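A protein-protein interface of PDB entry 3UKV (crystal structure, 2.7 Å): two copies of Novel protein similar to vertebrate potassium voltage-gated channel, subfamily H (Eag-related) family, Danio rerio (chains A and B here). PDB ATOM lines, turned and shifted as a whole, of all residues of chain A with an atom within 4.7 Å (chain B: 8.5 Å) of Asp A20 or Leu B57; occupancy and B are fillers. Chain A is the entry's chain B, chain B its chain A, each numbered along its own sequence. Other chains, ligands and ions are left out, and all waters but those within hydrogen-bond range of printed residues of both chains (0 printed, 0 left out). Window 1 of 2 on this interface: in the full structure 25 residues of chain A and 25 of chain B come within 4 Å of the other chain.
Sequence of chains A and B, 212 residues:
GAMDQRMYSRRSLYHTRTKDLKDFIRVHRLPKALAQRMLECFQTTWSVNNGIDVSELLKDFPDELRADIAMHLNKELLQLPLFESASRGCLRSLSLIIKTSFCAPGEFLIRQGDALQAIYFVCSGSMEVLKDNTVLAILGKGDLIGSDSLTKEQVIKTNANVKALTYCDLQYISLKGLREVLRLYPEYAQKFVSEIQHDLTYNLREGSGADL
3 positions are printed for both chains.
Printed residues of chain B within 4 Å of Arg A17: Leu B57.
Asp A20 touches one residue of chain B.
Of the printed residues of chain B, Leu A21 touches Leu B57.
Of the printed residues of chain B, Phe A24 touches Leu B58 and Ile B69.
Of the printed residues of chain A, Leu B58 touches Phe A24 (3.9 Å).
Of the printed residues of chain A, Ile B69 touches Phe A24.
The nearest printed residue of chain B that does not touch Leu A21 is Leu B58 (4.1 Å).
The guanidinium group (NH1) of Arg A17 is in salt-bridge range of the side-chain carboxylate (OD2) of Asp A20, at 3.8 Å.
The backbone carbonyl oxygen (O) of Leu B58 sits at hydrogen-bond distance from the guanidinium group (NH1) of Arg B66, 2.8 Å away.
Among the printed residues, pairs that only touch across the chains: Arg A17 with Leu B57, Asp A20 with Leu B57, Leu A21 with Leu B57, Phe A24 with Leu B58 and Phe A24 with Ile B69.
Of the 17 printed residues of chain B, 3 touch a printed residue of chain A.
Hydrophobic or aromatic side chains of chain B that line the printed part of chain A: Leu B57, Leu B58 and Ile B69.
Of the 9 printed residues of chain A, 4 touch a printed residue of chain B.
Printed residues of chain A that touch a printed residue of chain B: Arg A17, Asp A20, Leu A21 and Phe A24.
Hydrophobic or aromatic side chains of chain A that line the printed part of chain B: Leu A21 and Phe A24.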
ATOM      1  N   THR A  16      16.488 -32.992   3.264  1.00  0.00           N
ATOM      2  CA  THR A  16      16.283 -31.886   2.357  1.00  0.00           C
ATOM      3  C   THR A  16      17.440 -30.896   2.493  1.00  0.00           C
ATOM      4  O   THR A  16      18.015 -30.450   1.504  1.00  0.00           O
ATOM      5  CB  THR A  16      14.978 -31.158   2.685  1.00  0.00           C
ATOM      6  OG1 THR A  16      13.895 -32.072   2.599  1.00  0.00           O
ATOM      7  CG2 THR A  16      14.741 -29.997   1.715  1.00  0.00           C
ATOM      8  N   ARG A  17      17.767 -30.559   3.732  1.00  0.00           N
ATOM      9  CA  ARG A  17      18.870 -29.664   4.021  1.00  0.00           C
ATOM     10  C   ARG A  17      20.206 -30.248   3.585  1.00  0.00           C
ATOM     11  O   ARG A  17      21.060 -29.519   3.084  1.00  0.00           O
ATOM     12  CB  ARG A  17      18.903 -29.350   5.512  1.00  0.00           C
ATOM     13  CG  ARG A  17      18.258 -28.025   5.872  1.00  0.00           C
ATOM     14  CD  ARG A  17      17.095 -27.699   4.973  1.00  0.00           C
ATOM     15  NE  ARG A  17      16.425 -26.485   5.419  1.00  0.00           N
ATOM     16  CZ  ARG A  17      15.423 -25.902   4.766  1.00  0.00           C
ATOM     17  NH1 ARG A  17      14.969 -26.416   3.628  1.00  0.00           N
ATOM     18  NH2 ARG A  17      14.876 -24.805   5.256  1.00  0.00           N
ATOM     19  N   THR A  18      20.385 -31.553   3.792  1.00  0.00           N
ATOM     20  CA  THR A  18      21.582 -32.249   3.341  1.00  0.00           C
ATOM     21  C   THR A  18      21.713 -32.102   1.827  1.00  0.00           C
ATOM     22  O   THR A  18      22.801 -31.843   1.303  1.00  0.00           O
ATOM     23  CB  THR A  18      21.569 -33.758   3.736  1.00  0.00           C
ATOM     24  OG1 THR A  18      21.853 -33.902   5.134  1.00  0.00           O
ATOM     25  CG2 THR A  18      22.614 -34.538   2.955  1.00  0.00           C
ATOM     26  N   LYS A  19      20.595 -32.243   1.130  1.00  0.00           N
ATOM     27  CA  LYS A  19      20.602 -32.168  -0.325  1.00  0.00           C
ATOM     28  C   LYS A  19      20.819 -30.732  -0.850  1.00  0.00           C
ATOM     29  O   LYS A  19      21.407 -30.543  -1.904  1.00  0.00           O
ATOM     30  CB  LYS A  19      19.321 -32.792  -0.898  1.00  0.00           C
ATOM     31  CG  LYS A  19      19.209 -32.741  -2.401  1.00  0.00           C
ATOM     32  CD  LYS A  19      17.848 -33.248  -2.867  1.00  0.00           C
ATOM     33  N   ASP A  20      20.347 -29.727  -0.119  1.00  0.00           N
ATOM     34  CA  ASP A  20      20.618 -28.345  -0.479  1.00  0.00           C
ATOM     35  C   ASP A  20      22.105 -28.031  -0.349  1.00  0.00           C
ATOM     36  O   ASP A  20      22.697 -27.366  -1.202  1.00  0.00           O
ATOM     37  CB  ASP A  20      19.834 -27.389   0.415  1.00  0.00           C
ATOM     38  CG  ASP A  20      18.362 -27.360   0.092  1.00  0.00           C
ATOM     39  OD1 ASP A  20      17.982 -27.840  -0.997  1.00  0.00           O
ATOM     40  OD2 ASP A  20      17.586 -26.841   0.931  1.00  0.00           O
ATOM     41  N   LEU A  21      22.701 -28.498   0.741  1.00  0.00           N
ATOM     42  CA  LEU A  21      24.123 -28.335   0.951  1.00  0.00           C
ATOM     43  C   LEU A  21      24.908 -29.003  -0.170  1.00  0.00           C
ATOM     44  O   LEU A  21      25.895 -28.447  -0.658  1.00  0.00           O
ATOM     45  CB  LEU A  21      24.522 -28.936   2.286  1.00  0.00           C
ATOM     46  CG  LEU A  21      25.935 -28.640   2.760  1.00  0.00           C
ATOM     47  CD1 LEU A  21      26.243 -27.176   2.534  1.00  0.00           C
ATOM     48  CD2 LEU A  21      26.050 -28.992   4.226  1.00  0.00           C
ATOM     49  N   LYS A  22      24.471 -30.196  -0.577  1.00  0.00           N
ATOM     50  CA  LYS A  22      25.204 -30.959  -1.575  1.00  0.00           C
ATOM     51  C   LYS A  22      25.153 -30.300  -2.933  1.00  0.00           C
ATOM     52  O   LYS A  22      26.116 -30.385  -3.685  1.00  0.00           O
ATOM     53  CB  LYS A  22      24.724 -32.397  -1.643  1.00  0.00           C
ATOM     54  CG  LYS A  22      25.364 -33.264  -0.596  1.00  0.00           C
ATOM     55  CD  LYS A  22      24.865 -34.691  -0.691  1.00  0.00           C
ATOM     56  CE  LYS A  22      25.685 -35.618   0.193  1.00  0.00           C
ATOM     57  NZ  LYS A  22      24.885 -36.789   0.647  1.00  0.00           N
ATOM     58  N   ASP A  23      24.051 -29.629  -3.238  1.00  0.00           N
ATOM     59  CA  ASP A  23      23.987 -28.813  -4.448  1.00  0.00           C
ATOM     60  C   ASP A  23      24.882 -27.589  -4.338  1.00  0.00           C
ATOM     61  O   ASP A  23      25.657 -27.293  -5.239  1.00  0.00           O
ATOM     62  CB  ASP A  23      22.563 -28.348  -4.738  1.00  0.00           C
ATOM     63  CG  ASP A  23      21.643 -29.490  -5.108  1.00  0.00           C
ATOM     64  OD1 ASP A  23      22.140 -30.643  -5.243  1.00  0.00           O
ATOM     65  OD2 ASP A  23      20.424 -29.222  -5.263  1.00  0.00           O
ATOM     66  N   PHE A  24      24.764 -26.869  -3.237  1.00  0.00           N
ATOM     67  CA  PHE A  24      25.621 -25.726  -3.028  1.00  0.00           C
ATOM     68  C   PHE A  24      27.082 -26.124  -3.296  1.00  0.00           C
ATOM     69  O   PHE A  24      27.825 -25.412  -3.948  1.00  0.00           O
ATOM     70  CB  PHE A  24      25.456 -25.179  -1.608  1.00  0.00           C
ATOM     71  CG  PHE A  24      26.417 -24.089  -1.283  1.00  0.00           C
ATOM     72  CD1 PHE A  24      26.082 -22.768  -1.508  1.00  0.00           C
ATOM     73  CD2 PHE A  24      27.675 -24.378  -0.795  1.00  0.00           C
ATOM     74  CE1 PHE A  24      26.981 -21.742  -1.227  1.00  0.00           C
ATOM     75  CE2 PHE A  24      28.586 -23.360  -0.514  1.00  0.00           C
ATOM     76  CZ  PHE A  24      28.240 -22.044  -0.733  1.00  0.00           C
ATOM     77  N   THR B  16      11.621 -25.697  -8.428  1.00  0.00           N
ATOM     78  CA  THR B  16      11.716 -26.151  -7.040  1.00  0.00           C
ATOM     79  C   THR B  16      10.395 -25.921  -6.308  1.00  0.00           C
ATOM     80  O   THR B  16       9.870 -26.819  -5.656  1.00  0.00           O
ATOM     81  CB  THR B  16      12.829 -25.415  -6.248  1.00  0.00           C
ATOM     82  OG1 THR B  16      14.099 -25.655  -6.851  1.00  0.00           O
ATOM     83  CG2 THR B  16      12.877 -25.914  -4.823  1.00  0.00           C
ATOM     84  N   ARG B  17       9.865 -24.710  -6.413  1.00  0.00           N
ATOM     85  CA  ARG B  17       8.636 -24.348  -5.725  1.00  0.00           C
ATOM     86  C   ARG B  17       7.453 -25.156  -6.213  1.00  0.00           C
ATOM     87  O   ARG B  17       6.572 -25.507  -5.440  1.00  0.00           O
ATOM     88  CB  ARG B  17       8.358 -22.871  -5.926  1.00  0.00           C
ATOM     89  CG  ARG B  17       8.516 -22.065  -4.682  1.00  0.00           C
ATOM     90  CD  ARG B  17       9.752 -22.461  -3.914  1.00  0.00           C
ATOM     91  NE  ARG B  17      10.085 -21.452  -2.913  1.00  0.00           N
ATOM     92  CZ  ARG B  17      10.731 -21.703  -1.780  1.00  0.00           C
ATOM     93  NH1 ARG B  17      11.098 -22.957  -1.496  1.00  0.00           N
ATOM     94  NH2 ARG B  17      11.002 -20.708  -0.928  1.00  0.00           N
ATOM     95  N   ASP B  20       7.665 -28.430  -4.493  1.00  0.00           N
ATOM     96  CA  ASP B  20       7.100 -28.264  -3.161  1.00  0.00           C
ATOM     97  C   ASP B  20       5.564 -28.422  -3.211  1.00  0.00           C
ATOM     98  O   ASP B  20       4.953 -29.077  -2.358  1.00  0.00           O
ATOM     99  CB  ASP B  20       7.426 -26.873  -2.591  1.00  0.00           C
ATOM    100  CG  ASP B  20       8.924 -26.658  -2.289  1.00  0.00           C
ATOM    101  OD1 ASP B  20       9.706 -27.642  -2.194  1.00  0.00           O
ATOM    102  OD2 ASP B  20       9.297 -25.464  -2.117  1.00  0.00           O
ATOM    103  N   ASP B  53      14.693 -18.003  -1.934  1.00  0.00           N
ATOM    104  CA  ASP B  53      15.404 -18.853  -0.972  1.00  0.00           C
ATOM    105  C   ASP B  53      15.909 -18.064   0.263  1.00  0.00           C
ATOM    106  O   ASP B  53      16.816 -17.233   0.153  1.00  0.00           O
ATOM    107  CB  ASP B  53      16.577 -19.490  -1.700  1.00  0.00           C
ATOM    108  CG  ASP B  53      17.225 -20.596  -0.916  1.00  0.00           C
ATOM    109  OD1 ASP B  53      16.877 -20.776   0.272  1.00  0.00           O
ATOM    110  OD2 ASP B  53      18.097 -21.281  -1.507  1.00  0.00           O
ATOM    111  N   VAL B  54      15.329 -18.310   1.433  1.00  0.00           N
ATOM    112  CA  VAL B  54      15.663 -17.521   2.628  1.00  0.00           C
ATOM    113  C   VAL B  54      16.424 -18.304   3.708  1.00  0.00           C
ATOM    114  O   VAL B  54      16.822 -17.740   4.727  1.00  0.00           O
ATOM    115  CB  VAL B  54      14.407 -16.828   3.283  1.00  0.00           C
ATOM    116  CG1 VAL B  54      13.558 -16.120   2.236  1.00  0.00           C
ATOM    117  CG2 VAL B  54      13.570 -17.852   4.062  1.00  0.00           C
ATOM    118  N   SER B  55      16.621 -19.598   3.480  1.00  0.00           N
ATOM    119  CA  SER B  55      17.461 -20.428   4.339  1.00  0.00           C
ATOM    120  C   SER B  55      18.932 -19.947   4.380  1.00  0.00           C
ATOM    121  O   SER B  55      19.471 -19.467   3.385  1.00  0.00           O
ATOM    122  CB  SER B  55      17.406 -21.876   3.856  1.00  0.00           C
ATOM    123  OG  SER B  55      18.005 -21.998   2.575  1.00  0.00           O
ATOM    124  N   GLU B  56      19.574 -20.075   5.538  1.00  0.00           N
ATOM    125  CA  GLU B  56      20.986 -19.735   5.661  1.00  0.00           C
ATOM    126  C   GLU B  56      21.737 -20.955   6.180  1.00  0.00           C
ATOM    127  O   GLU B  56      22.052 -21.067   7.361  1.00  0.00           O
ATOM    128  CB  GLU B  56      21.189 -18.517   6.569  1.00  0.00           C
ATOM    129  CG  GLU B  56      22.518 -17.785   6.364  1.00  0.00           C
ATOM    130  CD  GLU B  56      22.709 -16.597   7.326  1.00  0.00           C
ATOM    131  OE1 GLU B  56      21.718 -15.846   7.562  1.00  0.00           O
ATOM    132  OE2 GLU B  56      23.853 -16.424   7.838  1.00  0.00           O
ATOM    133  N   LEU B  57      22.014 -21.874   5.266  1.00  0.00           N
ATOM    134  CA  LEU B  57      22.604 -23.165   5.589  1.00  0.00           C
ATOM    135  C   LEU B  57      23.964 -23.082   6.286  1.00  0.00           C
ATOM    136  O   LEU B  57      24.298 -23.954   7.079  1.00  0.00           O
ATOM    137  CB  LEU B  57      22.744 -23.968   4.302  1.00  0.00           C
ATOM    138  CG  LEU B  57      21.942 -25.256   4.138  1.00  0.00           C
ATOM    139  CD1 LEU B  57      20.448 -25.047   4.392  1.00  0.00           C
ATOM    140  CD2 LEU B  57      22.201 -25.803   2.746  1.00  0.00           C
ATOM    141  N   LEU B  58      24.751 -22.045   5.982  1.00  0.00           N
ATOM    142  CA  LEU B  58      26.116 -21.928   6.530  1.00  0.00           C
ATOM    143  C   LEU B  58      26.183 -21.026   7.765  1.00  0.00           C
ATOM    144  O   LEU B  58      27.258 -20.745   8.269  1.00  0.00           O
ATOM    145  CB  LEU B  58      27.121 -21.435   5.474  1.00  0.00           C
ATOM    146  CG  LEU B  58      26.940 -21.885   4.015  1.00  0.00           C
ATOM    147  CD1 LEU B  58      28.035 -21.344   3.105  1.00  0.00           C
ATOM    148  CD2 LEU B  58      26.857 -23.403   3.876  1.00  0.00           C
ATOM    149  N   LYS B  59      25.032 -20.578   8.248  1.00  0.00           N
ATOM    150  CA  LYS B  59      24.993 -19.641   9.362  1.00  0.00           C
ATOM    151  C   LYS B  59      25.762 -20.128  10.590  1.00  0.00           C
ATOM    152  O   LYS B  59      26.473 -19.352  11.218  1.00  0.00           O
ATOM    153  CB  LYS B  59      23.548 -19.327   9.737  1.00  0.00           C
ATOM    154  CG  LYS B  59      23.383 -18.373  10.896  1.00  0.00           C
ATOM    155  CD  LYS B  59      21.925 -18.376  11.359  1.00  0.00           C
ATOM    156  CE  LYS B  59      21.663 -17.310  12.410  1.00  0.00           C
ATOM    157  NZ  LYS B  59      22.069 -15.954  11.953  1.00  0.00           N
ATOM    158  N   ASP B  60      25.631 -21.407  10.929  1.00  0.00           N
ATOM    159  CA  ASP B  60      26.197 -21.903  12.181  1.00  0.00           C
ATOM    160  C   ASP B  60      27.548 -22.602  12.042  1.00  0.00           C
ATOM    161  O   ASP B  60      27.942 -23.356  12.926  1.00  0.00           O
ATOM    162  CB  ASP B  60      25.214 -22.840  12.881  1.00  0.00           C
ATOM    163  CG  ASP B  60      23.968 -22.122  13.382  1.00  0.00           C
ATOM    164  OD1 ASP B  60      24.048 -20.901  13.644  1.00  0.00           O
ATOM    165  OD2 ASP B  60      22.908 -22.783  13.518  1.00  0.00           O
ATOM    166  N   PHE B  61      28.254 -22.363  10.944  1.00  0.00           N
ATOM    167  CA  PHE B  61      29.567 -22.963  10.737  1.00  0.00           C
ATOM    168  C   PHE B  61      30.650 -22.136  11.426  1.00  0.00           C
ATOM    169  O   PHE B  61      30.535 -20.895  11.494  1.00  0.00           O
ATOM    170  CB  PHE B  61      29.888 -23.047   9.240  1.00  0.00           C
ATOM    171  CG  PHE B  61      29.157 -24.142   8.513  1.00  0.00           C
ATOM    172  CD1 PHE B  61      28.167 -24.884   9.142  1.00  0.00           C
ATOM    173  CD2 PHE B  61      29.475 -24.447   7.195  1.00  0.00           C
ATOM    174  CE1 PHE B  61      27.502 -25.903   8.463  1.00  0.00           C
ATOM    175  CE2 PHE B  61      28.812 -25.466   6.514  1.00  0.00           C
ATOM    176  CZ  PHE B  61      27.833 -26.195   7.152  1.00  0.00           C
ATOM    177  N   ARG B  66      33.867 -21.065   7.420  1.00  0.00           N
ATOM    178  CA  ARG B  66      33.171 -20.065   6.641  1.00  0.00           C
ATOM    179  C   ARG B  66      34.118 -19.237   5.770  1.00  0.00           C
ATOM    180  O   ARG B  66      33.834 -18.992   4.599  1.00  0.00           O
ATOM    181  CB  ARG B  66      32.316 -19.189   7.556  1.00  0.00           C
ATOM    182  CG  ARG B  66      31.072 -19.917   8.081  1.00  0.00           C
ATOM    183  CD  ARG B  66      30.366 -19.071   9.122  1.00  0.00           C
ATOM    184  NE  ARG B  66      30.168 -17.728   8.588  1.00  0.00           N
ATOM    185  CZ  ARG B  66      29.027 -17.278   8.068  1.00  0.00           C
ATOM    186  NH1 ARG B  66      27.952 -18.054   8.010  1.00  0.00           N
ATOM    187  NH2 ARG B  66      28.971 -16.033   7.600  1.00  0.00           N
ATOM    188  N   ILE B  69      35.076 -21.464   2.711  1.00  0.00           N
ATOM    189  CA  ILE B  69      34.040 -21.517   1.689  1.00  0.00           C
ATOM    190  C   ILE B  69      33.988 -20.215   0.886  1.00  0.00           C
ATOM    191  O   ILE B  69      33.892 -20.247  -0.350  1.00  0.00           O
ATOM    192  CB  ILE B  69      32.644 -21.814   2.286  1.00  0.00           C
ATOM    193  CG1 ILE B  69      32.664 -23.122   3.070  1.00  0.00           C
ATOM    194  CG2 ILE B  69      31.595 -21.905   1.187  1.00  0.00           C
ATOM    195  CD1 ILE B  69      31.368 -23.425   3.790  1.00  0.00           C
ATOM    196  N   LEU B  96      28.512 -15.184   1.329  1.00  0.00           N
ATOM    197  CA  LEU B  96      27.950 -16.429   1.835  1.00  0.00           C
ATOM    198  C   LEU B  96      26.413 -16.462   1.814  1.00  0.00           C
ATOM    199  O   LEU B  96      25.826 -17.549   1.804  1.00  0.00           O
ATOM    200  CB  LEU B  96      28.507 -16.754   3.216  1.00  0.00           C
ATOM    201  CG  LEU B  96      29.990 -17.157   3.197  1.00  0.00           C
ATOM    202  CD1 LEU B  96      30.544 -17.387   4.596  1.00  0.00           C
ATOM    203  CD2 LEU B  96      30.208 -18.386   2.343  1.00  0.00           C
ATOM    204  N   ILE B  97      25.763 -15.291   1.770  1.00  0.00           N
ATOM    205  CA  ILE B  97      24.298 -15.233   1.668  1.00  0.00           C
ATOM    206  C   ILE B  97      23.715 -14.866   0.303  1.00  0.00           C
ATOM    207  O   ILE B  97      22.533 -14.565   0.200  1.00  0.00           O
ATOM    208  CB  ILE B  97      23.673 -14.296   2.699  1.00  0.00           C
ATOM    209  CG1 ILE B  97      24.084 -12.846   2.450  1.00  0.00           C
ATOM    210  CG2 ILE B  97      24.005 -14.768   4.112  1.00  0.00           C
ATOM    211  CD1 ILE B  97      23.438 -11.905   3.421  1.00  0.00           C
ATOM    212  N   LYS B  99      22.160 -15.628  -3.206  1.00  0.00           N
ATOM    213  CA  LYS B  99      21.451 -16.728  -3.847  1.00  0.00           C
ATOM    214  C   LYS B  99      21.377 -16.508  -5.346  1.00  0.00           C
ATOM    215  O   LYS B  99      21.581 -15.393  -5.825  1.00  0.00           O
ATOM    216  CB  LYS B  99      20.050 -16.851  -3.268  1.00  0.00           C
ATOM    217  CG  LYS B  99      20.020 -16.959  -1.768  1.00  0.00           C
ATOM    218  CD  LYS B  99      20.349 -18.361  -1.344  1.00  0.00           C
ATOM    219  CE  LYS B  99      19.838 -18.639   0.053  1.00  0.00           C
ATOM    220  NZ  LYS B  99      19.999 -20.072   0.416  1.00  0.00           N
